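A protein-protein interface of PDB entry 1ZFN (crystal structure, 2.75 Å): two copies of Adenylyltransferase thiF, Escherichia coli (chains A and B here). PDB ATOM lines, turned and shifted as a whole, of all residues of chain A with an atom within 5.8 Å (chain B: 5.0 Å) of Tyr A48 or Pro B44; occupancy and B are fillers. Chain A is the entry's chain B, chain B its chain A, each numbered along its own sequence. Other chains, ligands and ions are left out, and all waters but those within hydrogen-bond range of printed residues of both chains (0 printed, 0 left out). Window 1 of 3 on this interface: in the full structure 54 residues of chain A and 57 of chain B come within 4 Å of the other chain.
The side-chain amide oxygen of Gln B71 lies close to the side-chain amide oxygen of Gln A14 (2.9 Å).
O of Ala A52 is in hydrogen-bond range of NE2 of Gln A14 (3.2 Å). The side-chain hydroxyl (OG1) of Thr B201 sits close to the backbone carbonyl oxygen (O) of Gly B197 (3.3 Å). The guanidinium group (NE) of Arg B72 sits close to the side-chain amide nitrogen (NE2) of Gln B71, at 3.1 Å.
Pro A44 touches Tyr B48. Ile B74 touches Leu A47 (CG2 to CG, 3.6 Å). Arg B72 touches Tyr A48. Tyr A48 touches Gly B193 (CE2 to O, 3.6 Å). OH of Tyr A48 touches CA of Gly B197 (3.2 Å). Gly A51 touches Gln B71. Ile A74 touches Leu B47. Tyr B48 touches Ile A74 (OH to CD1, 3.9 Å). CG2 of Thr A201 touches O of Pro B194, at 3.2 Å. Ile A208 touches Pro B194 (CD1 to CD, 3.8 Å).
Tyr A48 touches just these residues of chain B: Pro B44, Arg B72, Ile B74, Gly B193, Pro B194 and Gly B197. Pro B44 touches just one residue of chain A: Tyr A48. Of the printed residues of chain A, Arg B72 touches Tyr A48. Of the printed residues of chain B, Gly A51 touches Gln B71. Printed residues of chain A within 4 Å of Gly B193: Tyr A48 (3.6 Å). Leu B41 touches none of the printed residues of chain A. Ala B45 touches none of the printed residues of chain A. The nearest residue of chain B that does not touch Tyr A48 is Gln B71 (4.7 Å). The nearest residue of chain A that does not touch Pro B44 is Ile A74 (5.6 Å). The nearest printed residue of chain B that does not touch Thr A201 is Gly B197 (4.2 Å).
Of the 16 printed residues of chain A, 9 touch a printed residue of chain B. Hydrophobic or aromatic side chains of chain A that line the printed part of chain B: Pro A44, Leu A47, Tyr A48, Ile A74, Ala A204 and Ile A208. Along chain A the printed residues that touch a printed residue of chain B span positions 14 to 208. Along chain B the printed residues that touch a printed residue of chain A span positions 44 to 197. Among the printed residues, no Asp or Glu carboxylate lies within 4 Å of a Lys or Arg side-chain nitrogen of the other chain.
Pro A44 touches Tyr B48, and with the chains exchanged Tyr A48 touches Pro B44. Leu A47 touches Ile B74, and with the chains exchanged Ile A74 touches Leu B47. Tyr A48 touches Ile B74, and with the chains exchanged Ile A74 touches Tyr B48. Ile B74 touches its own counterpart, Ile A74. 9 positions are printed for both chains.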
ATOM      1  N   GLN A  14     -11.886 -11.246  19.616  1.00  0.00           N
ATOM      2  CA  GLN A  14     -11.574 -10.908  18.228  1.00  0.00           C
ATOM      3  C   GLN A  14     -10.608 -11.981  17.719  1.00  0.00           C
ATOM      4  O   GLN A  14     -10.777 -12.534  16.624  1.00  0.00           O
ATOM      5  CB  GLN A  14     -10.869  -9.555  18.131  1.00  0.00           C
ATOM      6  CG  GLN A  14     -11.681  -8.381  18.585  1.00  0.00           C
ATOM      7  CD  GLN A  14     -10.945  -7.066  18.439  1.00  0.00           C
ATOM      8  OE1 GLN A  14     -11.533  -6.004  18.636  1.00  0.00           O
ATOM      9  NE2 GLN A  14      -9.660  -7.122  18.102  1.00  0.00           N
ATOM     10  N   THR A  43     -16.655  10.272  19.080  1.00  0.00           N
ATOM     11  CA  THR A  43     -16.700   9.732  20.424  1.00  0.00           C
ATOM     12  C   THR A  43     -16.825   8.209  20.447  1.00  0.00           C
ATOM     13  O   THR A  43     -15.904   7.522  20.885  1.00  0.00           O
ATOM     14  CB  THR A  43     -17.820  10.442  21.258  1.00  0.00           C
ATOM     15  OG1 THR A  43     -17.204  11.406  22.121  1.00  0.00           O
ATOM     16  CG2 THR A  43     -18.612   9.476  22.099  1.00  0.00           C
ATOM     17  N   PRO A  44     -17.951   7.656  19.965  1.00  0.00           N
ATOM     18  CA  PRO A  44     -18.049   6.196  19.994  1.00  0.00           C
ATOM     19  C   PRO A  44     -16.945   5.562  19.148  1.00  0.00           C
ATOM     20  O   PRO A  44     -16.415   4.520  19.491  1.00  0.00           O
ATOM     21  CB  PRO A  44     -19.444   5.940  19.426  1.00  0.00           C
ATOM     22  CG  PRO A  44     -19.587   7.041  18.432  1.00  0.00           C
ATOM     23  CD  PRO A  44     -19.079   8.235  19.215  1.00  0.00           C
ATOM     24  N   ALA A  45     -16.595   6.202  18.042  1.00  0.00           N
ATOM     25  CA  ALA A  45     -15.561   5.666  17.182  1.00  0.00           C
ATOM     26  C   ALA A  45     -14.253   5.474  17.944  1.00  0.00           C
ATOM     27  O   ALA A  45     -13.729   4.373  18.004  1.00  0.00           O
ATOM     28  CB  ALA A  45     -15.345   6.580  15.975  1.00  0.00           C
ATOM     29  N   ALA A  46     -13.717   6.535  18.523  1.00  0.00           N
ATOM     30  CA  ALA A  46     -12.468   6.394  19.254  1.00  0.00           C
ATOM     31  C   ALA A  46     -12.595   5.283  20.286  1.00  0.00           C
ATOM     32  O   ALA A  46     -11.698   4.460  20.439  1.00  0.00           O
ATOM     33  CB  ALA A  46     -12.092   7.705  19.933  1.00  0.00           C
ATOM     34  N   LEU A  47     -13.724   5.253  20.981  1.00  0.00           N
ATOM     35  CA  LEU A  47     -13.968   4.246  22.007  1.00  0.00           C
ATOM     36  C   LEU A  47     -13.824   2.810  21.471  1.00  0.00           C
ATOM     37  O   LEU A  47     -13.108   1.996  22.050  1.00  0.00           O
ATOM     38  CB  LEU A  47     -15.363   4.466  22.601  1.00  0.00           C
ATOM     39  CG  LEU A  47     -15.595   4.346  24.110  1.00  0.00           C
ATOM     40  CD1 LEU A  47     -14.448   4.960  24.868  1.00  0.00           C
ATOM     41  CD2 LEU A  47     -16.894   5.051  24.478  1.00  0.00           C
ATOM     42  N   TYR A  48     -14.487   2.500  20.360  1.00  0.00           N
ATOM     43  CA  TYR A  48     -14.416   1.162  19.784  1.00  0.00           C
ATOM     44  C   TYR A  48     -13.067   0.790  19.164  1.00  0.00           C
ATOM     45  O   TYR A  48     -12.682  -0.379  19.172  1.00  0.00           O
ATOM     46  CB  TYR A  48     -15.529   0.970  18.747  1.00  0.00           C
ATOM     47  CG  TYR A  48     -16.878   0.699  19.375  1.00  0.00           C
ATOM     48  CD1 TYR A  48     -17.885   1.659  19.367  1.00  0.00           C
ATOM     49  CD2 TYR A  48     -17.129  -0.499  20.029  1.00  0.00           C
ATOM     50  CE1 TYR A  48     -19.109   1.431  20.003  1.00  0.00           C
ATOM     51  CE2 TYR A  48     -18.341  -0.732  20.665  1.00  0.00           C
ATOM     52  CZ  TYR A  48     -19.325   0.240  20.650  1.00  0.00           C
ATOM     53  OH  TYR A  48     -20.514   0.023  21.314  1.00  0.00           O
ATOM     54  N   LEU A  49     -12.355   1.770  18.622  1.00  0.00           N
ATOM     55  CA  LEU A  49     -11.064   1.493  18.022  1.00  0.00           C
ATOM     56  C   LEU A  49     -10.012   1.254  19.101  1.00  0.00           C
ATOM     57  O   LEU A  49      -9.061   0.507  18.888  1.00  0.00           O
ATOM     58  CB  LEU A  49     -10.638   2.638  17.104  1.00  0.00           C
ATOM     59  CG  LEU A  49     -11.405   2.763  15.779  1.00  0.00           C
ATOM     60  CD1 LEU A  49     -10.818   3.893  14.960  1.00  0.00           C
ATOM     61  CD2 LEU A  49     -11.336   1.454  14.984  1.00  0.00           C
ATOM     62  N   ALA A  50     -10.191   1.887  20.257  1.00  0.00           N
ATOM     63  CA  ALA A  50      -9.274   1.733  21.381  1.00  0.00           C
ATOM     64  C   ALA A  50      -9.537   0.372  22.010  1.00  0.00           C
ATOM     65  O   ALA A  50      -8.607  -0.374  22.345  1.00  0.00           O
ATOM     66  CB  ALA A  50      -9.509   2.831  22.405  1.00  0.00           C
ATOM     67  N   GLY A  51     -10.811   0.050  22.171  1.00  0.00           N
ATOM     68  CA  GLY A  51     -11.161  -1.236  22.734  1.00  0.00           C
ATOM     69  C   GLY A  51     -10.681  -2.374  21.843  1.00  0.00           C
ATOM     70  O   GLY A  51     -10.291  -3.431  22.344  1.00  0.00           O
ATOM     71  N   ALA A  52     -10.708  -2.155  20.529  1.00  0.00           N
ATOM     72  CA  ALA A  52     -10.275  -3.156  19.550  1.00  0.00           C
ATOM     73  C   ALA A  52      -8.774  -3.364  19.570  1.00  0.00           C
ATOM     74  O   ALA A  52      -8.275  -4.391  19.098  1.00  0.00           O
ATOM     75  CB  ALA A  52     -10.695  -2.742  18.149  1.00  0.00           C
ATOM     76  N   GLY A  53      -8.056  -2.380  20.100  1.00  0.00           N
ATOM     77  CA  GLY A  53      -6.617  -2.472  20.161  1.00  0.00           C
ATOM     78  C   GLY A  53      -5.904  -1.898  18.953  1.00  0.00           C
ATOM     79  O   GLY A  53      -4.978  -2.513  18.422  1.00  0.00           O
ATOM     80  N   ILE A  74     -20.920  10.143  24.312  1.00  0.00           N
ATOM     81  CA  ILE A  74     -20.739   9.144  25.366  1.00  0.00           C
ATOM     82  C   ILE A  74     -19.380   8.990  26.081  1.00  0.00           C
ATOM     83  O   ILE A  74     -19.304   8.379  27.147  1.00  0.00           O
ATOM     84  CB  ILE A  74     -21.178   7.765  24.825  1.00  0.00           C
ATOM     85  CG1 ILE A  74     -20.439   7.467  23.521  1.00  0.00           C
ATOM     86  CG2 ILE A  74     -22.670   7.766  24.530  1.00  0.00           C
ATOM     87  CD1 ILE A  74     -20.433   6.034  23.128  1.00  0.00           C
ATOM     88  N   THR A 201     -20.022   4.376  15.381  1.00  0.00           N
ATOM     89  CA  THR A 201     -19.628   2.995  15.581  1.00  0.00           C
ATOM     90  C   THR A 201     -19.347   2.345  14.231  1.00  0.00           C
ATOM     91  O   THR A 201     -18.439   1.532  14.108  1.00  0.00           O
ATOM     92  CB  THR A 201     -20.723   2.234  16.320  1.00  0.00           C
ATOM     93  OG1 THR A 201     -20.930   2.851  17.597  1.00  0.00           O
ATOM     94  CG2 THR A 201     -20.324   0.790  16.526  1.00  0.00           C
ATOM     95  N   ALA A 204     -15.993   3.012  12.837  1.00  0.00           N
ATOM     96  CA  ALA A 204     -15.026   2.156  13.512  1.00  0.00           C
ATOM     97  C   ALA A 204     -14.977   0.757  12.880  1.00  0.00           C
ATOM     98  O   ALA A 204     -13.904   0.215  12.637  1.00  0.00           O
ATOM     99  CB  ALA A 204     -15.367   2.057  14.991  1.00  0.00           C
ATOM    100  N   ILE A 208     -11.585  -0.957  11.241  1.00  0.00           N
ATOM    101  CA  ILE A 208     -11.068  -2.237  11.682  1.00  0.00           C
ATOM    102  C   ILE A 208     -10.981  -3.172  10.471  1.00  0.00           C
ATOM    103  O   ILE A 208      -9.935  -3.765  10.213  1.00  0.00           O
ATOM    104  CB  ILE A 208     -11.985  -2.870  12.759  1.00  0.00           C
ATOM    105  CG1 ILE A 208     -11.838  -2.121  14.087  1.00  0.00           C
ATOM    106  CG2 ILE A 208     -11.649  -4.359  12.908  1.00  0.00           C
ATOM    107  CD1 ILE A 208     -12.856  -2.511  15.129  1.00  0.00           C
ATOM    108  N   GLY B  39     -23.686  -5.809  28.968  1.00  0.00           N
ATOM    109  CA  GLY B  39     -22.507  -6.224  28.245  1.00  0.00           C
ATOM    110  C   GLY B  39     -22.289  -5.422  26.975  1.00  0.00           C
ATOM    111  O   GLY B  39     -22.287  -4.192  26.999  1.00  0.00           O
ATOM    112  N   GLY B  40     -22.114  -6.129  25.863  1.00  0.00           N
ATOM    113  CA  GLY B  40     -21.865  -5.488  24.585  1.00  0.00           C
ATOM    114  C   GLY B  40     -23.033  -4.716  24.023  1.00  0.00           C
ATOM    115  O   GLY B  40     -22.836  -3.724  23.334  1.00  0.00           O
ATOM    116  N   LEU B  41     -24.244  -5.178  24.295  1.00  0.00           N
ATOM    117  CA  LEU B  41     -25.438  -4.495  23.812  1.00  0.00           C
ATOM    118  C   LEU B  41     -25.904  -3.449  24.826  1.00  0.00           C
ATOM    119  O   LEU B  41     -26.060  -2.276  24.487  1.00  0.00           O
ATOM    120  CB  LEU B  41     -26.568  -5.490  23.585  1.00  0.00           C
ATOM    121  CG  LEU B  41     -26.443  -6.592  22.534  1.00  0.00           C
ATOM    122  CD1 LEU B  41     -27.472  -7.659  22.881  1.00  0.00           C
ATOM    123  CD2 LEU B  41     -26.659  -6.060  21.115  1.00  0.00           C
ATOM    124  N   GLY B  42     -26.105  -3.883  26.070  1.00  0.00           N
ATOM    125  CA  GLY B  42     -26.574  -2.989  27.115  1.00  0.00           C
ATOM    126  C   GLY B  42     -25.714  -1.781  27.429  1.00  0.00           C
ATOM    127  O   GLY B  42     -26.225  -0.693  27.651  1.00  0.00           O
ATOM    128  N   THR B  43     -24.403  -1.964  27.450  1.00  0.00           N
ATOM    129  CA  THR B  43     -23.479  -0.883  27.766  1.00  0.00           C
ATOM    130  C   THR B  43     -23.681   0.364  26.897  1.00  0.00           C
ATOM    131  O   THR B  43     -23.783   1.470  27.412  1.00  0.00           O
ATOM    132  CB  THR B  43     -22.014  -1.424  27.706  1.00  0.00           C
ATOM    133  OG1 THR B  43     -21.479  -1.434  29.029  1.00  0.00           O
ATOM    134  CG2 THR B  43     -21.122  -0.607  26.804  1.00  0.00           C
ATOM    135  N   PRO B  44     -23.743   0.211  25.568  1.00  0.00           N
ATOM    136  CA  PRO B  44     -23.945   1.425  24.779  1.00  0.00           C
ATOM    137  C   PRO B  44     -25.413   1.874  24.826  1.00  0.00           C
ATOM    138  O   PRO B  44     -25.708   3.057  24.698  1.00  0.00           O
ATOM    139  CB  PRO B  44     -23.505   0.995  23.383  1.00  0.00           C
ATOM    140  CG  PRO B  44     -23.946  -0.417  23.340  1.00  0.00           C
ATOM    141  CD  PRO B  44     -23.487  -0.941  24.688  1.00  0.00           C
ATOM    142  N   ALA B  45     -26.323   0.921  25.012  1.00  0.00           N
ATOM    143  CA  ALA B  45     -27.755   1.217  25.078  1.00  0.00           C
ATOM    144  C   ALA B  45     -28.049   2.127  26.263  1.00  0.00           C
ATOM    145  O   ALA B  45     -28.720   3.145  26.124  1.00  0.00           O
ATOM    146  CB  ALA B  45     -28.589  -0.100  25.201  1.00  0.00           C
ATOM    147  N   ALA B  46     -27.538   1.735  27.425  1.00  0.00           N
ATOM    148  CA  ALA B  46     -27.718   2.474  28.662  1.00  0.00           C
ATOM    149  C   ALA B  46     -27.100   3.850  28.551  1.00  0.00           C
ATOM    150  O   ALA B  46     -27.617   4.817  29.097  1.00  0.00           O
ATOM    151  CB  ALA B  46     -27.076   1.721  29.807  1.00  0.00           C
ATOM    152  N   LEU B  47     -25.981   3.924  27.842  1.00  0.00           N
ATOM    153  CA  LEU B  47     -25.267   5.173  27.647  1.00  0.00           C
ATOM    154  C   LEU B  47     -26.076   6.197  26.854  1.00  0.00           C
ATOM    155  O   LEU B  47     -26.220   7.344  27.272  1.00  0.00           O
ATOM    156  CB  LEU B  47     -23.960   4.898  26.923  1.00  0.00           C
ATOM    157  CG  LEU B  47     -22.768   5.625  27.525  1.00  0.00           C
ATOM    158  CD1 LEU B  47     -22.715   5.329  29.015  1.00  0.00           C
ATOM    159  CD2 LEU B  47     -21.492   5.176  26.835  1.00  0.00           C
ATOM    160  N   TYR B  48     -26.601   5.777  25.708  1.00  0.00           N
ATOM    161  CA  TYR B  48     -27.372   6.658  24.860  1.00  0.00           C
ATOM    162  C   TYR B  48     -28.741   7.003  25.434  1.00  0.00           C
ATOM    163  O   TYR B  48     -29.283   8.081  25.150  1.00  0.00           O
ATOM    164  CB  TYR B  48     -27.512   6.055  23.455  1.00  0.00           C
ATOM    165  CG  TYR B  48     -26.305   6.286  22.572  1.00  0.00           C
ATOM    166  CD1 TYR B  48     -25.288   5.331  22.466  1.00  0.00           C
ATOM    167  CD2 TYR B  48     -26.150   7.489  21.885  1.00  0.00           C
ATOM    168  CE1 TYR B  48     -24.139   5.569  21.698  1.00  0.00           C
ATOM    169  CE2 TYR B  48     -25.008   7.744  21.119  1.00  0.00           C
ATOM    170  CZ  TYR B  48     -23.999   6.778  21.029  1.00  0.00           C
ATOM    171  OH  TYR B  48     -22.860   7.051  20.290  1.00  0.00           O
ATOM    172  N   LEU B  49     -29.308   6.108  26.236  1.00  0.00           N
ATOM    173  CA  LEU B  49     -30.612   6.386  26.824  1.00  0.00           C
ATOM    174  C   LEU B  49     -30.477   7.395  27.956  1.00  0.00           C
ATOM    175  O   LEU B  49     -31.358   8.231  28.159  1.00  0.00           O
ATOM    176  CB  LEU B  49     -31.273   5.108  27.340  1.00  0.00           C
ATOM    177  CG  LEU B  49     -31.947   4.243  26.269  1.00  0.00           C
ATOM    178  CD1 LEU B  49     -32.715   3.089  26.936  1.00  0.00           C
ATOM    179  CD2 LEU B  49     -32.893   5.093  25.434  1.00  0.00           C
ATOM    180  N   GLN B  71     -13.132  -4.784  25.367  1.00  0.00           N
ATOM    181  CA  GLN B  71     -12.897  -4.633  23.942  1.00  0.00           C
ATOM    182  C   GLN B  71     -14.167  -4.123  23.267  1.00  0.00           C
ATOM    183  O   GLN B  71     -14.126  -3.692  22.111  1.00  0.00           O
ATOM    184  CB  GLN B  71     -12.481  -5.961  23.303  1.00  0.00           C
ATOM    185  CG  GLN B  71     -13.599  -6.998  23.174  1.00  0.00           C
ATOM    186  CD  GLN B  71     -14.030  -7.208  21.735  1.00  0.00           C
ATOM    187  OE1 GLN B  71     -13.266  -6.965  20.805  1.00  0.00           O
ATOM    188  NE2 GLN B  71     -15.246  -7.679  21.545  1.00  0.00           N
ATOM    189  N   ARG B  72     -15.288  -4.150  23.986  1.00  0.00           N
ATOM    190  CA  ARG B  72     -16.541  -3.718  23.383  1.00  0.00           C
ATOM    191  C   ARG B  72     -17.595  -3.152  24.347  1.00  0.00           C
ATOM    192  O   ARG B  72     -18.599  -2.560  23.915  1.00  0.00           O
ATOM    193  CB  ARG B  72     -17.143  -4.894  22.617  1.00  0.00           C
ATOM    194  CG  ARG B  72     -17.843  -5.892  23.518  1.00  0.00           C
ATOM    195  CD  ARG B  72     -18.045  -7.216  22.844  1.00  0.00           C
ATOM    196  NE  ARG B  72     -17.401  -8.247  23.642  1.00  0.00           N
ATOM    197  CZ  ARG B  72     -18.055  -9.139  24.373  1.00  0.00           C
ATOM    198  NH1 ARG B  72     -19.389  -9.136  24.394  1.00  0.00           N
ATOM    199  NH2 ARG B  72     -17.371 -10.005  25.118  1.00  0.00           N
ATOM    200  N   ILE B  74     -17.947  -0.531  26.123  1.00  0.00           N
ATOM    201  CA  ILE B  74     -17.488   0.846  26.251  1.00  0.00           C
ATOM    202  C   ILE B  74     -17.753   1.637  27.534  1.00  0.00           C
ATOM    203  O   ILE B  74     -17.090   2.638  27.781  1.00  0.00           O
ATOM    204  CB  ILE B  74     -18.028   1.661  25.090  1.00  0.00           C
ATOM    205  CG1 ILE B  74     -19.542   1.475  25.021  1.00  0.00           C
ATOM    206  CG2 ILE B  74     -17.350   1.224  23.797  1.00  0.00           C
ATOM    207  CD1 ILE B  74     -20.248   2.413  24.094  1.00  0.00           C
ATOM    208  N   GLY B 193     -16.477  -5.796  18.160  1.00  0.00           N
ATOM    209  CA  GLY B 193     -16.952  -4.649  18.923  1.00  0.00           C
ATOM    210  C   GLY B 193     -17.996  -3.772  18.244  1.00  0.00           C
ATOM    211  O   GLY B 193     -19.140  -3.692  18.694  1.00  0.00           O
ATOM    212  N   PRO B 194     -17.622  -3.074  17.170  1.00  0.00           N
ATOM    213  CA  PRO B 194     -18.586  -2.223  16.482  1.00  0.00           C
ATOM    214  C   PRO B 194     -19.879  -2.935  16.075  1.00  0.00           C
ATOM    215  O   PRO B 194     -20.949  -2.331  16.083  1.00  0.00           O
ATOM    216  CB  PRO B 194     -17.787  -1.712  15.292  1.00  0.00           C
ATOM    217  CG  PRO B 194     -16.453  -1.533  15.890  1.00  0.00           C
ATOM    218  CD  PRO B 194     -16.264  -2.818  16.669  1.00  0.00           C
ATOM    219  N   GLY B 197     -21.957  -3.207  19.004  1.00  0.00           N
ATOM    220  CA  GLY B 197     -22.186  -1.821  19.372  1.00  0.00           C
ATOM    221  C   GLY B 197     -23.338  -1.219  18.590  1.00  0.00           C
ATOM    222  O   GLY B 197     -24.249  -0.628  19.159  1.00  0.00           O
ATOM    223  N   GLY B 200     -26.708  -2.588  20.053  1.00  0.00           N
ATOM    224  CA  GLY B 200     -27.194  -2.055  21.318  1.00  0.00           C
ATOM    225  C   GLY B 200     -27.646  -0.612  21.123  1.00  0.00           C
ATOM    226  O   GLY B 200     -28.682  -0.185  21.634  1.00  0.00           O
ATOM    227  N   THR B 201     -26.848   0.141  20.376  1.00  0.00           N
ATOM    228  CA  THR B 201     -27.162   1.520  20.088  1.00  0.00           C
ATOM    229  C   THR B 201     -28.513   1.598  19.375  1.00  0.00           C
ATOM    230  O   THR B 201     -29.310   2.499  19.647  1.00  0.00           O
ATOM    231  CB  THR B 201     -26.060   2.146  19.232  1.00  0.00           C
ATOM    232  OG1 THR B 201     -24.956   2.481  20.082  1.00  0.00           O
ATOM    233  CG2 THR B 201     -26.568   3.385  18.493  1.00  0.00           C
